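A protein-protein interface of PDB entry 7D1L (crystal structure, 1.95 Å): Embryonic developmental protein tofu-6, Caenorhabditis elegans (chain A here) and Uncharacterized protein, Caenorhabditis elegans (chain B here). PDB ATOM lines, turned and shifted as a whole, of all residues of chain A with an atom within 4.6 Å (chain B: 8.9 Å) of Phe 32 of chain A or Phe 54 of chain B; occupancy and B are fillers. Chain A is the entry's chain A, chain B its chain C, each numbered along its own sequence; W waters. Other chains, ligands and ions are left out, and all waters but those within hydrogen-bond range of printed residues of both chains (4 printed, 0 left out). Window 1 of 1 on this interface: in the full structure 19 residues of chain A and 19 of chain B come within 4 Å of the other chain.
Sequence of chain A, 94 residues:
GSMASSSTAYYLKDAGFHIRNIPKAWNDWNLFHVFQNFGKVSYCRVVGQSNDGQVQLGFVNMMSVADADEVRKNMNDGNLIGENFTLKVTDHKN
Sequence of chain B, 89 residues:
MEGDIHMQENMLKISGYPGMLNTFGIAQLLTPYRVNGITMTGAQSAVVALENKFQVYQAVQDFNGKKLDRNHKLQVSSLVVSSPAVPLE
The side-chain sulfur of Cys 44 of chain A sits at hydrogen-bond distance from the backbone carbonyl oxygen of Asp 28 of chain A (3.2 Å). The backbone NH of Phe 32 of chain A sits at hydrogen-bond distance from the side-chain sulfur of Cys 44 of chain A. OD1 of Asn 52 of chain B lies within hydrogen-bond range of N of Phe 54 of chain B, 3.0 Å away. The side-chain amide oxygen of Asn 52 of chain B is in hydrogen-bond range of the backbone NH of Gln 55 of chain B. OG of Ser 78 of chain B lies within hydrogen-bond range of N of Val 80 of chain B (3.1 Å).
Water W3 lies within hydrogen-bond range of the side-chain amide oxygen (OE1) of Gln 36 of chain A (2.7 Å), the side-chain hydroxyl (OH) of Tyr 57 of chain B (3.0 Å) and the side-chain amide nitrogen (NE2) of Gln 61 of chain B (3.1 Å). Water W1 bridges OD1 of Asp 28 of chain A and NZ of Lys 53 of chain B. Water W2 lies within hydrogen-bond range of the indole nitrogen (NE1) of Trp 29 of chain A (3.1 Å) and the side-chain amino group (NZ) of Lys 53 of chain B (3.2 Å).
Hydrophobic or aromatic side chains of chain B within 4 Å of the printed part of chain A: Phe 54, Tyr 57, Val 80, Pro 84 and Leu 88. Along chain B the printed residues that touch a printed residue of chain A span positions 53 to 88. Among the printed residues, Asp or Glu carboxylates within 4 Å of a Lys or Arg side-chain nitrogen of the other chain: Asp 28 of chain A with Lys 53 of chain B.
Trp 29 of chain A touches Ser 83 of chain B (CG to N, 3.4 Å). Pro 84 of chain B touches Trp 29 of chain A. Asn 30 of chain A touches Leu 88 of chain B. Phe 32 of chain A touches Phe 54 of chain B (CD1 to CD1, 3.5 Å). Tyr 57 of chain B touches Phe 32 of chain A (CE2 to CE2, 3.8 Å). Phe 32 of chain A touches Gln 58 of chain B (CE1 to NE2, 3.6 Å). CE1 of His 33 of chain A touches OH of Tyr 57 of chain B (3.5 Å). Val 41 of chain A touches Gln 55 of chain B. CE2 of Phe 54 of chain B touches O of Cys 44 of chain A, at 3.4 Å.
The side-chain amino group (NZ) of Lys 53 of chain B lies within salt-bridge range of the side-chain carboxylate (OD2) of Asp 28 of chain A (2.7 Å). The side-chain hydroxyl (OG) of Ser 82 of chain B lies within hydrogen-bond range of a ring nitrogen (NE2) of His 33 of chain A (2.5 Å). The side-chain amide nitrogen of Gln 36 of chain A is in hydrogen-bond range of the side-chain amide oxygen of Gln 61 of chain B, at 2.8 Å. The side-chain amide nitrogen of Gln 58 of chain B sits at hydrogen-bond distance from the backbone carbonyl oxygen of Val 41 of chain A (2.8 Å).
Of the printed residues of chain B, Asp 28 of chain A touches Lys 53 (2.7 Å) and Phe 54 (3.6 Å). Of chain B, only Tyr 57, Ser 82 and Leu 88 come within 4 Å of His 33 of chain A. Of the printed residues of chain B, Gln 36 of chain A touches Gln 58 (3.8 Å) and Gln 61 (2.8 Å). Cys 44 of chain A touches just one residue of chain B: Phe 54 (3.4 Å). Of chain A, only Asp 28, Trp 29, Phe 32 and Cys 44 come within 4 Å of Phe 54 of chain B. Printed residues of chain A within 4 Å of Gln 58 of chain B: Phe 32, Gln 36 and Val 41. Ser 78 of chain B touches none of the printed residues of chain A. The nearest residue of chain B that does not touch Phe 32 of chain A is Gln 61 of chain B (5.7 Å). The nearest printed residue of chain A that does not touch Phe 54 of chain B is Val 41 of chain A (4.6 Å).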
ATOM      1  N   ASP A  28      -6.073  13.763  14.328  1.00  0.00           N
ATOM      2  CA  ASP A  28      -5.135  14.015  15.427  1.00  0.00           C
ATOM      3  C   ASP A  28      -4.638  12.720  16.070  1.00  0.00           C
ATOM      4  O   ASP A  28      -3.471  12.625  16.472  1.00  0.00           O
ATOM      5  CB  ASP A  28      -5.777  14.925  16.478  1.00  0.00           C
ATOM      6  CG  ASP A  28      -7.156  14.445  16.929  1.00  0.00           C
ATOM      7  OD1 ASP A  28      -7.619  13.364  16.484  1.00  0.00           O
ATOM      8  OD2 ASP A  28      -7.776  15.177  17.738  1.00  0.00           O
ATOM      9  N   TRP A  29      -5.504  11.707  16.172  1.00  0.00           N
ATOM     10  CA  TRP A  29      -5.070  10.414  16.709  1.00  0.00           C
ATOM     11  C   TRP A  29      -3.937   9.804  15.896  1.00  0.00           C
ATOM     12  O   TRP A  29      -3.010   9.210  16.465  1.00  0.00           O
ATOM     13  CB  TRP A  29      -6.253   9.451  16.776  1.00  0.00           C
ATOM     14  CG  TRP A  29      -7.072   9.681  17.998  1.00  0.00           C
ATOM     15  CD1 TRP A  29      -8.343  10.173  18.058  1.00  0.00           C
ATOM     16  CD2 TRP A  29      -6.672   9.425  19.344  1.00  0.00           C
ATOM     17  NE1 TRP A  29      -8.761  10.231  19.365  1.00  0.00           N
ATOM     18  CE2 TRP A  29      -7.748   9.785  20.174  1.00  0.00           C
ATOM     19  CE3 TRP A  29      -5.503   8.928  19.928  1.00  0.00           C
ATOM     20  CZ2 TRP A  29      -7.693   9.667  21.557  1.00  0.00           C
ATOM     21  CZ3 TRP A  29      -5.452   8.808  21.301  1.00  0.00           C
ATOM     22  CH2 TRP A  29      -6.537   9.174  22.100  1.00  0.00           C
ATOM     23  N   ASN A  30      -4.000   9.916  14.565  1.00  0.00           N
ATOM     24  CA  ASN A  30      -2.903   9.438  13.726  1.00  0.00           C
ATOM     25  C   ASN A  30      -1.608  10.174  14.054  1.00  0.00           C
ATOM     26  O   ASN A  30      -0.554   9.553  14.231  1.00  0.00           O
ATOM     27  CB  ASN A  30      -3.255   9.595  12.238  1.00  0.00           C
ATOM     28  CG  ASN A  30      -4.166   8.489  11.735  1.00  0.00           C
ATOM     29  OD1 ASN A  30      -5.334   8.722  11.410  1.00  0.00           O
ATOM     30  ND2 ASN A  30      -3.639   7.269  11.678  1.00  0.00           N
ATOM     31  N   LEU A  31      -1.672  11.503  14.154  1.00  0.00           N
ATOM     32  CA  LEU A  31      -0.476  12.270  14.499  1.00  0.00           C
ATOM     33  C   LEU A  31       0.030  11.896  15.884  1.00  0.00           C
ATOM     34  O   LEU A  31       1.240  11.719  16.085  1.00  0.00           O
ATOM     35  CB  LEU A  31      -0.769  13.764  14.437  1.00  0.00           C
ATOM     36  CG  LEU A  31       0.407  14.704  14.674  1.00  0.00           C
ATOM     37  CD1 LEU A  31       1.546  14.463  13.670  1.00  0.00           C
ATOM     38  CD2 LEU A  31      -0.087  16.141  14.592  1.00  0.00           C
ATOM     39  N   PHE A  32      -0.890  11.758  16.842  1.00  0.00           N
ATOM     40  CA  PHE A  32      -0.523  11.443  18.218  1.00  0.00           C
ATOM     41  C   PHE A  32       0.296  10.161  18.289  1.00  0.00           C
ATOM     42  O   PHE A  32       1.343  10.112  18.950  1.00  0.00           O
ATOM     43  CB  PHE A  32      -1.785  11.326  19.083  1.00  0.00           C
ATOM     44  CG  PHE A  32      -1.566  10.589  20.379  1.00  0.00           C
ATOM     45  CD1 PHE A  32      -1.119  11.263  21.508  1.00  0.00           C
ATOM     46  CD2 PHE A  32      -1.811   9.224  20.471  1.00  0.00           C
ATOM     47  CE1 PHE A  32      -0.905  10.581  22.710  1.00  0.00           C
ATOM     48  CE2 PHE A  32      -1.607   8.540  21.654  1.00  0.00           C
ATOM     49  CZ  PHE A  32      -1.156   9.218  22.785  1.00  0.00           C
ATOM     50  N   HIS A  33      -0.166   9.106  17.608  1.00  0.00           N
ATOM     51  CA  HIS A  33       0.505   7.822  17.748  1.00  0.00           C
ATOM     52  C   HIS A  33       1.910   7.853  17.164  1.00  0.00           C
ATOM     53  O   HIS A  33       2.788   7.115  17.628  1.00  0.00           O
ATOM     54  CB  HIS A  33      -0.347   6.708  17.114  1.00  0.00           C
ATOM     55  CG  HIS A  33      -1.472   6.258  17.994  1.00  0.00           C
ATOM     56  ND1 HIS A  33      -1.261   5.601  19.189  1.00  0.00           N
ATOM     57  CD2 HIS A  33      -2.814   6.415  17.883  1.00  0.00           C
ATOM     58  CE1 HIS A  33      -2.427   5.353  19.766  1.00  0.00           C
ATOM     59  NE2 HIS A  33      -3.385   5.840  18.996  1.00  0.00           N
ATOM     60  N   VAL A  34       2.166   8.712  16.179  1.00  0.00           N
ATOM     61  CA  VAL A  34       3.534   8.843  15.688  1.00  0.00           C
ATOM     62  C   VAL A  34       4.440   9.356  16.797  1.00  0.00           C
ATOM     63  O   VAL A  34       5.520   8.810  17.046  1.00  0.00           O
ATOM     64  CB  VAL A  34       3.582   9.761  14.457  1.00  0.00           C
ATOM     65  CG1 VAL A  34       5.024  10.076  14.100  1.00  0.00           C
ATOM     66  CG2 VAL A  34       2.860   9.103  13.287  1.00  0.00           C
ATOM     67  N   PHE A  35       4.014  10.418  17.484  1.00  0.00           N
ATOM     68  CA  PHE A  35       4.885  11.030  18.475  1.00  0.00           C
ATOM     69  C   PHE A  35       4.882  10.282  19.797  1.00  0.00           C
ATOM     70  O   PHE A  35       5.872  10.358  20.534  1.00  0.00           O
ATOM     71  CB  PHE A  35       4.497  12.494  18.665  1.00  0.00           C
ATOM     72  CG  PHE A  35       4.972  13.352  17.536  1.00  0.00           C
ATOM     73  CD1 PHE A  35       4.337  13.303  16.299  1.00  0.00           C
ATOM     74  CD2 PHE A  35       6.105  14.127  17.674  1.00  0.00           C
ATOM     75  CE1 PHE A  35       4.803  14.041  15.231  1.00  0.00           C
ATOM     76  CE2 PHE A  35       6.571  14.891  16.605  1.00  0.00           C
ATOM     77  CZ  PHE A  35       5.918  14.844  15.389  1.00  0.00           C
ATOM     78  N   GLN A  36       3.805   9.548  20.105  1.00  0.00           N
ATOM     79  CA  GLN A  36       3.774   8.793  21.353  1.00  0.00           C
ATOM     80  C   GLN A  36       4.854   7.719  21.379  1.00  0.00           C
ATOM     81  O   GLN A  36       5.305   7.321  22.456  1.00  0.00           O
ATOM     82  CB  GLN A  36       2.398   8.161  21.582  1.00  0.00           C
ATOM     83  CG  GLN A  36       2.241   7.647  23.030  1.00  0.00           C
ATOM     84  CD  GLN A  36       1.171   6.584  23.211  1.00  0.00           C
ATOM     85  OE1 GLN A  36       0.705   5.968  22.244  1.00  0.00           O
ATOM     86  NE2 GLN A  36       0.780   6.357  24.466  1.00  0.00           N
ATOM     87  N   VAL A  41       2.900  12.763  25.194  1.00  0.00           N
ATOM     88  CA  VAL A  41       2.417  13.849  24.350  1.00  0.00           C
ATOM     89  C   VAL A  41       1.426  14.689  25.140  1.00  0.00           C
ATOM     90  O   VAL A  41       0.448  14.156  25.676  1.00  0.00           O
ATOM     91  CB  VAL A  41       1.760  13.303  23.072  1.00  0.00           C
ATOM     92  CG1 VAL A  41       1.066  14.446  22.311  1.00  0.00           C
ATOM     93  CG2 VAL A  41       2.799  12.593  22.214  1.00  0.00           C
ATOM     94  N   CYS A  44      -1.885  17.720  20.632  1.00  0.00           N
ATOM     95  CA  CYS A  44      -1.653  17.396  19.284  1.00  0.00           C
ATOM     96  C   CYS A  44      -2.858  17.762  18.430  1.00  0.00           C
ATOM     97  O   CYS A  44      -3.975  17.576  18.810  1.00  0.00           O
ATOM     98  CB  CYS A  44      -1.306  15.928  19.311  1.00  0.00           C
ATOM     99  SG  CYS A  44      -1.794  14.959  17.957  1.00  0.00           S
ATOM    100  N   GLU B   9     -14.477  13.617  27.300  1.00  0.00           N
ATOM    101  CA  GLU B   9     -13.200  13.069  26.870  1.00  0.00           C
ATOM    102  C   GLU B   9     -12.023  13.555  27.707  1.00  0.00           C
ATOM    103  O   GLU B   9     -10.897  13.094  27.469  1.00  0.00           O
ATOM    104  CB  GLU B   9     -12.964  13.396  25.392  1.00  0.00           C
ATOM    105  CG  GLU B   9     -13.067  14.870  25.014  1.00  0.00           C
ATOM    106  CD  GLU B   9     -12.751  15.095  23.536  1.00  0.00           C
ATOM    107  OE1 GLU B   9     -13.342  14.380  22.694  1.00  0.00           O
ATOM    108  OE2 GLU B   9     -11.909  15.967  23.213  1.00  0.00           O
ATOM    109  N   ASN B  10     -12.238  14.456  28.667  1.00  0.00           N
ATOM    110  CA  ASN B  10     -11.183  14.896  29.584  1.00  0.00           C
ATOM    111  C   ASN B  10     -11.257  14.214  30.949  1.00  0.00           C
ATOM    112  O   ASN B  10     -10.382  14.443  31.797  1.00  0.00           O
ATOM    113  CB  ASN B  10     -11.246  16.413  29.768  1.00  0.00           C
ATOM    114  CG  ASN B  10     -11.049  17.170  28.464  1.00  0.00           C
ATOM    115  OD1 ASN B  10     -10.517  16.630  27.497  1.00  0.00           O
ATOM    116  ND2 ASN B  10     -11.475  18.424  28.435  1.00  0.00           N
ATOM    117  N   LEU B  12     -11.516  11.055  33.784  1.00  0.00           N
ATOM    118  CA  LEU B  12     -11.250   9.657  34.073  1.00  0.00           C
ATOM    119  C   LEU B  12     -11.686   9.351  35.493  1.00  0.00           C
ATOM    120  O   LEU B  12     -11.908  10.250  36.306  1.00  0.00           O
ATOM    121  CB  LEU B  12      -9.766   9.295  33.880  1.00  0.00           C
ATOM    122  CG  LEU B  12      -8.738  10.014  34.762  1.00  0.00           C
ATOM    123  CD1 LEU B  12      -8.590   9.369  36.129  1.00  0.00           C
ATOM    124  CD2 LEU B  12      -7.382  10.005  34.045  1.00  0.00           C
ATOM    125  N   TYR B  33       0.989  14.317  33.993  1.00  0.00           N
ATOM    126  CA  TYR B  33      -0.115  14.855  33.211  1.00  0.00           C
ATOM    127  C   TYR B  33      -0.735  16.066  33.896  1.00  0.00           C
ATOM    128  O   TYR B  33      -0.699  16.207  35.124  1.00  0.00           O
ATOM    129  CB  TYR B  33      -1.159  13.763  32.954  1.00  0.00           C
ATOM    130  CG  TYR B  33      -0.529  12.616  32.227  1.00  0.00           C
ATOM    131  CD1 TYR B  33      -0.158  12.746  30.896  1.00  0.00           C
ATOM    132  CD2 TYR B  33      -0.223  11.421  32.890  1.00  0.00           C
ATOM    133  CE1 TYR B  33       0.465  11.705  30.213  1.00  0.00           C
ATOM    134  CE2 TYR B  33       0.389  10.365  32.215  1.00  0.00           C
ATOM    135  CZ  TYR B  33       0.732  10.519  30.873  1.00  0.00           C
ATOM    136  OH  TYR B  33       1.356   9.500  30.183  1.00  0.00           O
ATOM    137  N   LEU B  50      -8.401  15.798  33.238  1.00  0.00           N
ATOM    138  CA  LEU B  50      -7.107  16.148  32.686  1.00  0.00           C
ATOM    139  C   LEU B  50      -7.280  17.142  31.548  1.00  0.00           C
ATOM    140  O   LEU B  50      -8.395  17.506  31.156  1.00  0.00           O
ATOM    141  CB  LEU B  50      -6.371  14.900  32.208  1.00  0.00           C
ATOM    142  CG  LEU B  50      -6.081  13.827  33.249  1.00  0.00           C
ATOM    143  CD1 LEU B  50      -5.159  12.793  32.631  1.00  0.00           C
ATOM    144  CD2 LEU B  50      -5.470  14.426  34.513  1.00  0.00           C
ATOM    145  N   GLU B  51      -6.149  17.550  30.974  1.00  0.00           N
ATOM    146  CA  GLU B  51      -6.164  18.643  30.010  1.00  0.00           C
ATOM    147  C   GLU B  51      -6.901  18.261  28.723  1.00  0.00           C
ATOM    148  O   GLU B  51      -7.619  19.088  28.150  1.00  0.00           O
ATOM    149  CB  GLU B  51      -4.727  19.082  29.720  1.00  0.00           C
ATOM    150  CG  GLU B  51      -4.582  20.045  28.559  1.00  0.00           C
ATOM    151  CD  GLU B  51      -5.189  21.409  28.845  1.00  0.00           C
ATOM    152  OE1 GLU B  51      -5.340  21.781  30.038  1.00  0.00           O
ATOM    153  OE2 GLU B  51      -5.521  22.113  27.869  1.00  0.00           O
ATOM    154  N   ASN B  52      -6.750  17.027  28.249  1.00  0.00           N
ATOM    155  CA  ASN B  52      -7.416  16.649  27.005  1.00  0.00           C
ATOM    156  C   ASN B  52      -7.422  15.130  26.884  1.00  0.00           C
ATOM    157  O   ASN B  52      -6.872  14.415  27.728  1.00  0.00           O
ATOM    158  CB  ASN B  52      -6.739  17.302  25.790  1.00  0.00           C
ATOM    159  CG  ASN B  52      -5.259  16.945  25.676  1.00  0.00           C
ATOM    160  OD1 ASN B  52      -4.876  15.778  25.787  1.00  0.00           O
ATOM    161  ND2 ASN B  52      -4.421  17.962  25.452  1.00  0.00           N
ATOM    162  N   LYS B  53      -8.029  14.649  25.793  1.00  0.00           N
ATOM    163  CA  LYS B  53      -8.241  13.219  25.616  1.00  0.00           C
ATOM    164  C   LYS B  53      -6.933  12.449  25.460  1.00  0.00           C
ATOM    165  O   LYS B  53      -6.863  11.282  25.859  1.00  0.00           O
ATOM    166  CB  LYS B  53      -9.148  12.976  24.408  1.00  0.00           C
ATOM    167  CG  LYS B  53      -8.461  13.269  23.053  1.00  0.00           C
ATOM    168  CD  LYS B  53      -9.456  13.357  21.899  1.00  0.00           C
ATOM    169  CE  LYS B  53      -8.707  13.691  20.589  1.00  0.00           C
ATOM    170  NZ  LYS B  53      -9.607  14.233  19.545  1.00  0.00           N
ATOM    171  N   PHE B  54      -5.894  13.059  24.873  1.00  0.00           N
ATOM    172  CA  PHE B  54      -4.629  12.336  24.736  1.00  0.00           C
ATOM    173  C   PHE B  54      -4.004  12.065  26.090  1.00  0.00           C
ATOM    174  O   PHE B  54      -3.428  10.992  26.313  1.00  0.00           O
ATOM    175  CB  PHE B  54      -3.642  13.111  23.864  1.00  0.00           C
ATOM    176  CG  PHE B  54      -4.183  13.446  22.528  1.00  0.00           C
ATOM    177  CD1 PHE B  54      -4.464  12.439  21.611  1.00  0.00           C
ATOM    178  CD2 PHE B  54      -4.439  14.758  22.185  1.00  0.00           C
ATOM    179  CE1 PHE B  54      -4.987  12.744  20.372  1.00  0.00           C
ATOM    180  CE2 PHE B  54      -4.952  15.066  20.935  1.00  0.00           C
ATOM    181  CZ  PHE B  54      -5.222  14.065  20.037  1.00  0.00           C
ATOM    182  N   GLN B  55      -4.079  13.039  26.997  1.00  0.00           N
ATOM    183  CA  GLN B  55      -3.497  12.826  28.314  1.00  0.00           C
ATOM    184  C   GLN B  55      -4.312  11.817  29.116  1.00  0.00           C
ATOM    185  O   GLN B  55      -3.741  10.989  29.832  1.00  0.00           O
ATOM    186  CB  GLN B  55      -3.364  14.166  29.035  1.00  0.00           C
ATOM    187  CG  GLN B  55      -2.331  15.084  28.368  1.00  0.00           C
ATOM    188  CD  GLN B  55      -1.952  16.276  29.230  1.00  0.00           C
ATOM    189  OE1 GLN B  55      -1.945  16.181  30.455  1.00  0.00           O
ATOM    190  NE2 GLN B  55      -1.630  17.415  28.586  1.00  0.00           N
ATOM    191  N   VAL B  56      -5.642  11.849  28.985  1.00  0.00           N
ATOM    192  CA  VAL B  56      -6.471  10.812  29.607  1.00  0.00           C
ATOM    193  C   VAL B  56      -6.075   9.434  29.083  1.00  0.00           C
ATOM    194  O   VAL B  56      -5.874   8.486  29.854  1.00  0.00           O
ATOM    195  CB  VAL B  56      -7.962  11.082  29.345  1.00  0.00           C
ATOM    196  CG1 VAL B  56      -8.781   9.810  29.665  1.00  0.00           C
ATOM    197  CG2 VAL B  56      -8.462  12.298  30.152  1.00  0.00           C
ATOM    198  N   TYR B  57      -5.983   9.304  27.753  1.00  0.00           N
ATOM    199  CA  TYR B  57      -5.606   8.032  27.145  1.00  0.00           C
ATOM    200  C   TYR B  57      -4.280   7.522  27.700  1.00  0.00           C
ATOM    201  O   TYR B  57      -4.148   6.344  28.041  1.00  0.00           O
ATOM    202  CB  TYR B  57      -5.523   8.199  25.630  1.00  0.00           C
ATOM    203  CG  TYR B  57      -4.995   6.999  24.876  1.00  0.00           C
ATOM    204  CD1 TYR B  57      -5.840   5.968  24.483  1.00  0.00           C
ATOM    205  CD2 TYR B  57      -3.657   6.921  24.518  1.00  0.00           C
ATOM    206  CE1 TYR B  57      -5.354   4.872  23.766  1.00  0.00           C
ATOM    207  CE2 TYR B  57      -3.159   5.840  23.796  1.00  0.00           C
ATOM    208  CZ  TYR B  57      -4.006   4.824  23.423  1.00  0.00           C
ATOM    209  OH  TYR B  57      -3.494   3.752  22.711  1.00  0.00           O
ATOM    210  N   GLN B  58      -3.275   8.396  27.768  1.00  0.00           N
ATOM    211  CA  GLN B  58      -1.967   7.971  28.255  1.00  0.00           C
ATOM    212  C   GLN B  58      -1.997   7.670  29.750  1.00  0.00           C
ATOM    213  O   GLN B  58      -1.330   6.740  30.212  1.00  0.00           O
ATOM    214  CB  GLN B  58      -0.925   9.043  27.957  1.00  0.00           C
ATOM    215  CG  GLN B  58      -0.632   9.229  26.463  1.00  0.00           C
ATOM    216  CD  GLN B  58       0.154  10.497  26.206  1.00  0.00           C
ATOM    217  OE1 GLN B  58       1.377  10.469  26.049  1.00  0.00           O
ATOM    218  NE2 GLN B  58      -0.544  11.625  26.174  1.00  0.00           N
ATOM    219  N   ALA B  59      -2.741   8.461  30.524  1.00  0.00           N
ATOM    220  CA  ALA B  59      -2.837   8.202  31.959  1.00  0.00           C
ATOM    221  C   ALA B  59      -3.480   6.840  32.244  1.00  0.00           C
ATOM    222  O   ALA B  59      -3.044   6.113  33.146  1.00  0.00           O
ATOM    223  CB  ALA B  59      -3.622   9.322  32.631  1.00  0.00           C
ATOM    224  N   VAL B  60      -4.528   6.483  31.500  1.00  0.00           N
ATOM    225  CA  VAL B  60      -5.138   5.167  31.682  1.00  0.00           C
ATOM    226  C   VAL B  60      -4.117   4.074  31.384  1.00  0.00           C
ATOM    227  O   VAL B  60      -3.977   3.109  32.142  1.00  0.00           O
ATOM    228  CB  VAL B  60      -6.399   5.022  30.806  1.00  0.00           C
ATOM    229  CG1 VAL B  60      -6.864   3.571  30.770  1.00  0.00           C
ATOM    230  CG2 VAL B  60      -7.522   5.917  31.312  1.00  0.00           C
ATOM    231  N   GLN B  61      -3.377   4.220  30.284  1.00  0.00           N
ATOM    232  CA  GLN B  61      -2.326   3.258  29.959  1.00  0.00           C
ATOM    233  C   GLN B  61      -1.287   3.178  31.075  1.00  0.00           C
ATOM    234  O   GLN B  61      -0.861   2.089  31.469  1.00  0.00           O
ATOM    235  CB  GLN B  61      -1.632   3.651  28.648  1.00  0.00           C
ATOM    236  CG  GLN B  61      -2.455   3.545  27.372  1.00  0.00           C
ATOM    237  CD  GLN B  61      -1.585   3.725  26.120  1.00  0.00           C
ATOM    238  OE1 GLN B  61      -0.730   4.617  26.065  1.00  0.00           O
ATOM    239  NE2 GLN B  61      -1.783   2.861  25.127  1.00  0.00           N
ATOM    240  N   ASP B  62      -0.845   4.334  31.577  1.00  0.00           N
ATOM    241  CA  ASP B  62       0.264   4.350  32.531  1.00  0.00           C
ATOM    242  C   ASP B  62      -0.153   3.812  33.893  1.00  0.00           C
ATOM    243  O   ASP B  62       0.641   3.165  34.579  1.00  0.00           O
ATOM    244  CB  ASP B  62       0.794   5.773  32.697  1.00  0.00           C
ATOM    245  CG  ASP B  62       1.606   6.237  31.510  1.00  0.00           C
ATOM    246  OD1 ASP B  62       1.724   5.479  30.526  1.00  0.00           O
ATOM    247  OD2 ASP B  62       2.121   7.372  31.574  1.00  0.00           O
ATOM    248  N   SER B  78     -11.630   5.307  31.572  1.00  0.00           N
ATOM    249  CA  SER B  78     -12.237   6.452  30.916  1.00  0.00           C
ATOM    250  C   SER B  78     -12.994   5.964  29.695  1.00  0.00           C
ATOM    251  O   SER B  78     -12.915   4.792  29.320  1.00  0.00           O
ATOM    252  CB  SER B  78     -11.188   7.486  30.513  1.00  0.00           C
ATOM    253  OG  SER B  78     -10.555   7.073  29.308  1.00  0.00           O
ATOM    254  N   VAL B  80     -12.359   7.450  26.788  1.00  0.00           N
ATOM    255  CA  VAL B  80     -11.521   7.855  25.666  1.00  0.00           C
ATOM    256  C   VAL B  80     -11.047   6.621  24.917  1.00  0.00           C
ATOM    257  O   VAL B  80     -10.493   5.691  25.515  1.00  0.00           O
ATOM    258  CB  VAL B  80     -10.335   8.701  26.151  1.00  0.00           C
ATOM    259  CG1 VAL B  80      -9.376   9.009  24.973  1.00  0.00           C
ATOM    260  CG2 VAL B  80     -10.847   9.982  26.785  1.00  0.00           C
ATOM    261  N   VAL B  81     -11.243   6.631  23.603  1.00  0.00           N
ATOM    262  CA  VAL B  81     -10.858   5.560  22.697  1.00  0.00           C
ATOM    263  C   VAL B  81      -9.934   6.155  21.646  1.00  0.00           C
ATOM    264  O   VAL B  81     -10.300   7.141  20.990  1.00  0.00           O
ATOM    265  CB  VAL B  81     -12.096   4.940  22.012  1.00  0.00           C
ATOM    266  CG1 VAL B  81     -11.693   3.796  21.092  1.00  0.00           C
ATOM    267  CG2 VAL B  81     -13.118   4.496  23.049  1.00  0.00           C
ATOM    268  N   SER B  82      -8.755   5.553  21.464  1.00  0.00           N
ATOM    269  CA  SER B  82      -7.915   5.928  20.330  1.00  0.00           C
ATOM    270  C   SER B  82      -8.669   5.670  19.034  1.00  0.00           C
ATOM    271  O   SER B  82      -9.129   4.551  18.784  1.00  0.00           O
ATOM    272  CB  SER B  82      -6.608   5.137  20.340  1.00  0.00           C
ATOM    273  OG  SER B  82      -5.865   5.352  19.140  1.00  0.00           O
ATOM    274  N   SER B  83      -8.796   6.704  18.201  1.00  0.00           N
ATOM    275  CA  SER B  83      -9.667   6.648  17.025  1.00  0.00           C
ATOM    276  C   SER B  83      -8.947   7.207  15.804  1.00  0.00           C
ATOM    277  O   SER B  83      -9.354   8.224  15.236  1.00  0.00           O
ATOM    278  CB  SER B  83     -10.964   7.414  17.293  1.00  0.00           C
ATOM    279  OG  SER B  83     -11.560   6.994  18.511  1.00  0.00           O
ATOM    280  N   PRO B  84      -7.863   6.559  15.368  1.00  0.00           N
ATOM    281  CA  PRO B  84      -7.164   7.038  14.172  1.00  0.00           C
ATOM    282  C   PRO B  84      -8.067   6.952  12.950  1.00  0.00           C
ATOM    283  O   PRO B  84      -8.839   5.999  12.789  1.00  0.00           O
ATOM    284  CB  PRO B  84      -5.965   6.090  14.052  1.00  0.00           C
ATOM    285  CG  PRO B  84      -6.399   4.851  14.758  1.00  0.00           C
ATOM    286  CD  PRO B  84      -7.258   5.324  15.899  1.00  0.00           C
ATOM    287  N   LEU B  88      -3.178   2.340  11.876  1.00  0.00           N
ATOM    288  CA  LEU B  88      -1.797   2.552  12.274  1.00  0.00           C
ATOM    289  C   LEU B  88      -0.874   1.643  11.470  1.00  0.00           C
ATOM    290  O   LEU B  88      -1.267   0.563  11.022  1.00  0.00           O
ATOM    291  CB  LEU B  88      -1.640   2.289  13.776  1.00  0.00           C
ATOM    292  CG  LEU B  88      -2.500   3.196  14.666  1.00  0.00           C
ATOM    293  CD1 LEU B  88      -2.179   3.021  16.149  1.00  0.00           C
ATOM    294  CD2 LEU B  88      -2.350   4.664  14.249  1.00  0.00           C
HETATM  295  O   HOH W   1     -10.410  13.101  16.536  1.00  0.00           O
HETATM  296  O   HOH W   2     -11.463  11.698  19.255  1.00  0.00           O
HETATM  297  O   HOH W   3      -0.554   3.626  22.403  1.00  0.00           O
HETATM  298  O   HOH W   4       2.595   8.022  26.441  1.00  0.00           O
